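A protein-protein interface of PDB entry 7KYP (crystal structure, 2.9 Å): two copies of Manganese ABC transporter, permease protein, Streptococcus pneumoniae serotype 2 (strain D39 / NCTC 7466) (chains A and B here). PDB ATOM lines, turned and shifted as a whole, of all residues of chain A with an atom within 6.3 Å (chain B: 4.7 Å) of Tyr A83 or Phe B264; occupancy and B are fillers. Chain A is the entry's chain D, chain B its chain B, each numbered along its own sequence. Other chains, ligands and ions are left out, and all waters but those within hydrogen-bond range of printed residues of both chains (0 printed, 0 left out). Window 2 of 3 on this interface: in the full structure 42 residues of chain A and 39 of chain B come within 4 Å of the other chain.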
ATOM      1  N   ALA A  78     -21.171 -21.873  12.093  1.00  0.00           N
ATOM      2  CA  ALA A  78     -22.309 -21.843  11.169  1.00  0.00           C
ATOM      3  C   ALA A  78     -21.910 -21.324   9.786  1.00  0.00           C
ATOM      4  O   ALA A  78     -22.414 -21.805   8.769  1.00  0.00           O
ATOM      5  CB  ALA A  78     -23.433 -20.997  11.744  1.00  0.00           C
ATOM      6  N   ILE A  79     -21.011 -20.340   9.760  1.00  0.00           N
ATOM      7  CA  ILE A  79     -20.480 -19.796   8.508  1.00  0.00           C
ATOM      8  C   ILE A  79     -19.589 -20.818   7.795  1.00  0.00           C
ATOM      9  O   ILE A  79     -19.644 -20.940   6.570  1.00  0.00           O
ATOM     10  CB  ILE A  79     -19.713 -18.472   8.748  1.00  0.00           C
ATOM     11  CG1 ILE A  79     -20.697 -17.360   9.126  1.00  0.00           C
ATOM     12  CG2 ILE A  79     -18.925 -18.054   7.509  1.00  0.00           C
ATOM     13  CD1 ILE A  79     -20.060 -16.175   9.821  1.00  0.00           C
ATOM     14  N   ILE A  80     -18.774 -21.549   8.558  1.00  0.00           N
ATOM     15  CA  ILE A  80     -17.924 -22.599   7.987  1.00  0.00           C
ATOM     16  C   ILE A  80     -18.760 -23.740   7.395  1.00  0.00           C
ATOM     17  O   ILE A  80     -18.425 -24.258   6.333  1.00  0.00           O
ATOM     18  CB  ILE A  80     -16.907 -23.150   9.021  1.00  0.00           C
ATOM     19  CG1 ILE A  80     -15.792 -22.125   9.251  1.00  0.00           C
ATOM     20  CG2 ILE A  80     -16.302 -24.470   8.549  1.00  0.00           C
ATOM     21  CD1 ILE A  80     -14.841 -22.471  10.379  1.00  0.00           C
ATOM     22  N   ILE A  81     -19.846 -24.118   8.068  1.00  0.00           N
ATOM     23  CA  ILE A  81     -20.698 -25.215   7.598  1.00  0.00           C
ATOM     24  C   ILE A  81     -21.247 -24.935   6.199  1.00  0.00           C
ATOM     25  O   ILE A  81     -21.094 -25.758   5.297  1.00  0.00           O
ATOM     26  CB  ILE A  81     -21.861 -25.506   8.575  1.00  0.00           C
ATOM     27  CG1 ILE A  81     -21.317 -26.131   9.860  1.00  0.00           C
ATOM     28  CG2 ILE A  81     -22.883 -26.448   7.946  1.00  0.00           C
ATOM     29  CD1 ILE A  81     -22.237 -26.002  11.055  1.00  0.00           C
ATOM     30  N   THR A  82     -21.872 -23.772   6.024  1.00  0.00           N
ATOM     31  CA  THR A  82     -22.421 -23.384   4.721  1.00  0.00           C
ATOM     32  C   THR A  82     -21.318 -23.220   3.672  1.00  0.00           C
ATOM     33  O   THR A  82     -21.530 -23.513   2.495  1.00  0.00           O
ATOM     34  CB  THR A  82     -23.241 -22.078   4.806  1.00  0.00           C
ATOM     35  OG1 THR A  82     -22.441 -21.039   5.382  1.00  0.00           O
ATOM     36  CG2 THR A  82     -24.495 -22.280   5.650  1.00  0.00           C
ATOM     37  N   TYR A  83     -20.148 -22.757   4.107  1.00  0.00           N
ATOM     38  CA  TYR A  83     -18.992 -22.607   3.221  1.00  0.00           C
ATOM     39  C   TYR A  83     -18.475 -23.956   2.710  1.00  0.00           C
ATOM     40  O   TYR A  83     -18.026 -24.051   1.566  1.00  0.00           O
ATOM     41  CB  TYR A  83     -17.867 -21.849   3.936  1.00  0.00           C
ATOM     42  CG  TYR A  83     -16.696 -21.499   3.042  1.00  0.00           C
ATOM     43  CD1 TYR A  83     -16.752 -20.401   2.188  1.00  0.00           C
ATOM     44  CD2 TYR A  83     -15.532 -22.266   3.053  1.00  0.00           C
ATOM     45  CE1 TYR A  83     -15.682 -20.077   1.368  1.00  0.00           C
ATOM     46  CE2 TYR A  83     -14.457 -21.949   2.237  1.00  0.00           C
ATOM     47  CZ  TYR A  83     -14.535 -20.854   1.398  1.00  0.00           C
ATOM     48  OH  TYR A  83     -13.471 -20.534   0.586  1.00  0.00           O
ATOM     49  N   ILE A  84     -18.536 -24.987   3.554  1.00  0.00           N
ATOM     50  CA  ILE A  84     -18.141 -26.343   3.153  1.00  0.00           C
ATOM     51  C   ILE A  84     -19.125 -26.900   2.121  1.00  0.00           C
ATOM     52  O   ILE A  84     -18.712 -27.513   1.138  1.00  0.00           O
ATOM     53  CB  ILE A  84     -18.053 -27.309   4.362  1.00  0.00           C
ATOM     54  CG1 ILE A  84     -16.959 -26.872   5.350  1.00  0.00           C
ATOM     55  CG2 ILE A  84     -17.796 -28.741   3.902  1.00  0.00           C
ATOM     56  CD1 ILE A  84     -15.541 -26.941   4.820  1.00  0.00           C
ATOM     57  N   LYS A  85     -20.419 -26.681   2.348  1.00  0.00           N
ATOM     58  CA  LYS A  85     -21.462 -27.139   1.424  1.00  0.00           C
ATOM     59  C   LYS A  85     -21.304 -26.505   0.043  1.00  0.00           C
ATOM     60  O   LYS A  85     -21.281 -27.202  -0.974  1.00  0.00           O
ATOM     61  CB  LYS A  85     -22.856 -26.800   1.958  1.00  0.00           C
ATOM     62  CG  LYS A  85     -23.250 -27.503   3.247  1.00  0.00           C
ATOM     63  CD  LYS A  85     -24.719 -27.255   3.569  1.00  0.00           C
ATOM     64  CE  LYS A  85     -24.965 -27.176   5.067  1.00  0.00           C
ATOM     65  NZ  LYS A  85     -26.414 -27.112   5.400  1.00  0.00           N
ATOM     66  N   GLY A  86     -21.199 -25.178   0.023  1.00  0.00           N
ATOM     67  CA  GLY A  86     -21.148 -24.416  -1.221  1.00  0.00           C
ATOM     68  C   GLY A  86     -19.878 -24.571  -2.038  1.00  0.00           C
ATOM     69  O   GLY A  86     -19.911 -24.414  -3.259  1.00  0.00           O
ATOM     70  N   ASN A  87     -18.760 -24.874  -1.379  1.00  0.00           N
ATOM     71  CA  ASN A  87     -17.461 -24.959  -2.055  1.00  0.00           C
ATOM     72  C   ASN A  87     -16.854 -26.365  -2.058  1.00  0.00           C
ATOM     73  O   ASN A  87     -15.644 -26.518  -2.249  1.00  0.00           O
ATOM     74  CB  ASN A  87     -16.475 -23.971  -1.422  1.00  0.00           C
ATOM     75  CG  ASN A  87     -16.938 -22.531  -1.535  1.00  0.00           C
ATOM     76  OD1 ASN A  87     -18.022 -22.177  -1.075  1.00  0.00           O
ATOM     77  ND2 ASN A  87     -16.111 -21.691  -2.149  1.00  0.00           N
ATOM     78  N   SER A  88     -17.681 -27.392  -1.864  1.00  0.00           N
ATOM     79  CA  SER A  88     -17.195 -28.772  -1.905  1.00  0.00           C
ATOM     80  C   SER A  88     -18.303 -29.798  -2.134  1.00  0.00           C
ATOM     81  O   SER A  88     -19.490 -29.466  -2.172  1.00  0.00           O
ATOM     82  CB  SER A  88     -16.437 -29.117  -0.617  1.00  0.00           C
ATOM     83  OG  SER A  88     -17.320 -29.486   0.428  1.00  0.00           O
ATOM     84  N   ILE A  90     -18.753 -32.281  -0.019  1.00  0.00           N
ATOM     85  CA  ILE A  90     -19.175 -32.744   1.310  1.00  0.00           C
ATOM     86  C   ILE A  90     -20.595 -32.270   1.645  1.00  0.00           C
ATOM     87  O   ILE A  90     -20.924 -31.093   1.488  1.00  0.00           O
ATOM     88  CB  ILE A  90     -18.170 -32.307   2.411  1.00  0.00           C
ATOM     89  CG1 ILE A  90     -16.975 -33.268   2.470  1.00  0.00           C
ATOM     90  CG2 ILE A  90     -18.822 -32.281   3.788  1.00  0.00           C
ATOM     91  CD1 ILE A  90     -16.123 -33.308   1.220  1.00  0.00           C
ATOM     92  N   LEU B 214     -12.436 -36.140  -1.067  1.00  0.00           N
ATOM     93  CA  LEU B 214     -11.978 -35.065  -1.952  1.00  0.00           C
ATOM     94  C   LEU B 214     -10.944 -35.529  -2.984  1.00  0.00           C
ATOM     95  O   LEU B 214     -10.751 -34.862  -4.000  1.00  0.00           O
ATOM     96  CB  LEU B 214     -11.383 -33.914  -1.131  1.00  0.00           C
ATOM     97  CG  LEU B 214     -12.298 -33.228  -0.110  1.00  0.00           C
ATOM     98  CD1 LEU B 214     -11.499 -32.264   0.754  1.00  0.00           C
ATOM     99  CD2 LEU B 214     -13.450 -32.510  -0.795  1.00  0.00           C
ATOM    100  N   PHE B 260      -7.883 -32.194   6.443  1.00  0.00           N
ATOM    101  CA  PHE B 260      -9.087 -31.829   5.701  1.00  0.00           C
ATOM    102  C   PHE B 260      -9.006 -30.387   5.205  1.00  0.00           C
ATOM    103  O   PHE B 260      -9.333 -30.106   4.054  1.00  0.00           O
ATOM    104  CB  PHE B 260     -10.337 -32.020   6.566  1.00  0.00           C
ATOM    105  CG  PHE B 260     -11.608 -31.560   5.907  1.00  0.00           C
ATOM    106  CD1 PHE B 260     -12.159 -32.278   4.855  1.00  0.00           C
ATOM    107  CD2 PHE B 260     -12.252 -30.406   6.337  1.00  0.00           C
ATOM    108  CE1 PHE B 260     -13.328 -31.857   4.242  1.00  0.00           C
ATOM    109  CE2 PHE B 260     -13.423 -29.980   5.730  1.00  0.00           C
ATOM    110  CZ  PHE B 260     -13.962 -30.706   4.682  1.00  0.00           C
ATOM    111  N   LEU B 261      -8.563 -29.483   6.078  1.00  0.00           N
ATOM    112  CA  LEU B 261      -8.427 -28.066   5.734  1.00  0.00           C
ATOM    113  C   LEU B 261      -7.424 -27.843   4.602  1.00  0.00           C
ATOM    114  O   LEU B 261      -7.692 -27.079   3.675  1.00  0.00           O
ATOM    115  CB  LEU B 261      -8.018 -27.253   6.970  1.00  0.00           C
ATOM    116  CG  LEU B 261      -7.827 -25.743   6.789  1.00  0.00           C
ATOM    117  CD1 LEU B 261      -9.043 -25.098   6.136  1.00  0.00           C
ATOM    118  CD2 LEU B 261      -7.532 -25.092   8.132  1.00  0.00           C
ATOM    119  N   ILE B 262      -6.272 -28.507   4.684  1.00  0.00           N
ATOM    120  CA  ILE B 262      -5.262 -28.436   3.624  1.00  0.00           C
ATOM    121  C   ILE B 262      -5.819 -29.030   2.327  1.00  0.00           C
ATOM    122  O   ILE B 262      -5.739 -28.404   1.269  1.00  0.00           O
ATOM    123  CB  ILE B 262      -3.953 -29.157   4.032  1.00  0.00           C
ATOM    124  CG1 ILE B 262      -3.247 -28.380   5.150  1.00  0.00           C
ATOM    125  CG2 ILE B 262      -3.013 -29.308   2.841  1.00  0.00           C
ATOM    126  CD1 ILE B 262      -2.211 -29.186   5.905  1.00  0.00           C
ATOM    127  N   SER B 263      -6.396 -30.225   2.425  1.00  0.00           N
ATOM    128  CA  SER B 263      -6.977 -30.916   1.270  1.00  0.00           C
ATOM    129  C   SER B 263      -8.161 -30.170   0.648  1.00  0.00           C
ATOM    130  O   SER B 263      -8.407 -30.291  -0.552  1.00  0.00           O
ATOM    131  CB  SER B 263      -7.421 -32.326   1.666  1.00  0.00           C
ATOM    132  OG  SER B 263      -6.344 -33.060   2.222  1.00  0.00           O
ATOM    133  N   PHE B 264      -8.888 -29.406   1.463  1.00  0.00           N
ATOM    134  CA  PHE B 264     -10.025 -28.611   0.985  1.00  0.00           C
ATOM    135  C   PHE B 264      -9.628 -27.623  -0.116  1.00  0.00           C
ATOM    136  O   PHE B 264     -10.443 -27.301  -0.981  1.00  0.00           O
ATOM    137  CB  PHE B 264     -10.671 -27.850   2.149  1.00  0.00           C
ATOM    138  CG  PHE B 264     -12.015 -27.260   1.822  1.00  0.00           C
ATOM    139  CD1 PHE B 264     -12.122 -25.971   1.318  1.00  0.00           C
ATOM    140  CD2 PHE B 264     -13.174 -27.992   2.030  1.00  0.00           C
ATOM    141  CE1 PHE B 264     -13.360 -25.426   1.021  1.00  0.00           C
ATOM    142  CE2 PHE B 264     -14.416 -27.453   1.736  1.00  0.00           C
ATOM    143  CZ  PHE B 264     -14.509 -26.168   1.231  1.00  0.00           C
ATOM    144  N   PHE B 265      -8.385 -27.143  -0.079  1.00  0.00           N
ATOM    145  CA  PHE B 265      -7.892 -26.183  -1.067  1.00  0.00           C
ATOM    146  C   PHE B 265      -7.019 -26.814  -2.157  1.00  0.00           C
ATOM    147  O   PHE B 265      -7.150 -26.459  -3.328  1.00  0.00           O
ATOM    148  CB  PHE B 265      -7.128 -25.052  -0.370  1.00  0.00           C
ATOM    149  CG  PHE B 265      -7.985 -24.217   0.544  1.00  0.00           C
ATOM    150  CD1 PHE B 265      -8.946 -23.361   0.021  1.00  0.00           C
ATOM    151  CD2 PHE B 265      -7.832 -24.284   1.923  1.00  0.00           C
ATOM    152  CE1 PHE B 265      -9.741 -22.589   0.855  1.00  0.00           C
ATOM    153  CE2 PHE B 265      -8.624 -23.515   2.762  1.00  0.00           C
ATOM    154  CZ  PHE B 265      -9.579 -22.667   2.227  1.00  0.00           C
ATOM    155  N   ILE B 266      -6.143 -27.747  -1.782  1.00  0.00           N
ATOM    156  CA  ILE B 266      -5.148 -28.291  -2.722  1.00  0.00           C
ATOM    157  C   ILE B 266      -5.590 -29.536  -3.510  1.00  0.00           C
ATOM    158  O   ILE B 266      -4.839 -30.019  -4.358  1.00  0.00           O
ATOM    159  CB  ILE B 266      -3.796 -28.592  -2.023  1.00  0.00           C
ATOM    160  CG1 ILE B 266      -3.866 -29.871  -1.174  1.00  0.00           C
ATOM    161  CG2 ILE B 266      -3.356 -27.400  -1.183  1.00  0.00           C
ATOM    162  CD1 ILE B 266      -2.538 -30.276  -0.570  1.00  0.00           C
ATOM    163  N   GLN B 270     -11.307 -30.214  -5.727  1.00  0.00           N
ATOM    164  CA  GLN B 270     -11.572 -28.933  -5.068  1.00  0.00           C
ATOM    165  C   GLN B 270     -11.083 -27.738  -5.889  1.00  0.00           C
ATOM    166  O   GLN B 270     -11.621 -26.637  -5.757  1.00  0.00           O
ATOM    167  CB  GLN B 270     -10.939 -28.895  -3.673  1.00  0.00           C
ATOM    168  CG  GLN B 270     -11.669 -29.739  -2.642  1.00  0.00           C
ATOM    169  CD  GLN B 270     -13.016 -29.154  -2.264  1.00  0.00           C
ATOM    170  OE1 GLN B 270     -14.059 -29.644  -2.693  1.00  0.00           O
ATOM    171  NE2 GLN B 270     -12.999 -28.090  -1.470  1.00  0.00           N
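The backbone carbonyl oxygen (O) of Asn A87 lies within hydrogen-bond range of the side-chain amide nitrogen (NE2) of Gln B270 (3.2 Å).
CE2 of Tyr A83 touches CE1 of Phe B264, at 3.8 Å. Phe B260 touches Ile A84. Phe B264 touches Ile A84 (CE2 to CD1, 3.3 Å). CZ of Phe B264 touches O of Asn A87 (3.7 Å). Ser A88 touches Phe B264 (CB to CE2, 3.5 Å). Gln B270 touches Ser A88 (OE1 to CB, 3.2 Å). Ile A90 touches Leu B214 (CD1 to CD2, 3.4 Å).
No position is printed for both chains.
Hydrophobic or aromatic side chains of chain A within 4 Å of the printed part of chain B: Tyr A83, Ile A84 and Ile A90.
Printed residues of chain B within 4 Å of Tyr A83: Phe B264 (3.8 Å). Of the printed residues of chain B, Ile A84 touches Phe B260 (3.8 Å) and Phe B264 (3.3 Å). Of the printed residues of chain B, Ser A88 touches Phe B264 (3.5 Å) and Gln B270 (3.2 Å). Of the printed residues of chain A, Leu B214 touches Ile A90. Of chain A, only Tyr A83 (3.8 Å), Ile A84 (3.3 Å), Asn A87 (3.7 Å) and Ser A88 (3.5 Å) come within 4 Å of Phe B264. Printed residues of chain A within 4 Å of Gln B270: Asn A87 (3.2 Å) and Ser A88 (3.2 Å). The nearest residue of chain B that does not touch Tyr A83 is Phe B265 (4.3 Å).
The backbone carbonyl oxygen of Phe B264 lies within hydrogen-bond range of the side-chain amide nitrogen of Gln B270, 2.7 Å away. O of Tyr A83 sits close to OD1 of Asn A87 (3.2 Å). OG of Ser A88 is in hydrogen-bond range of O of Ile A84, 2.5 Å away. The backbone NH (N) of Ile A90 is in hydrogen-bond range of the side-chain hydroxyl (OG) of Ser A88 (3.2 Å).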
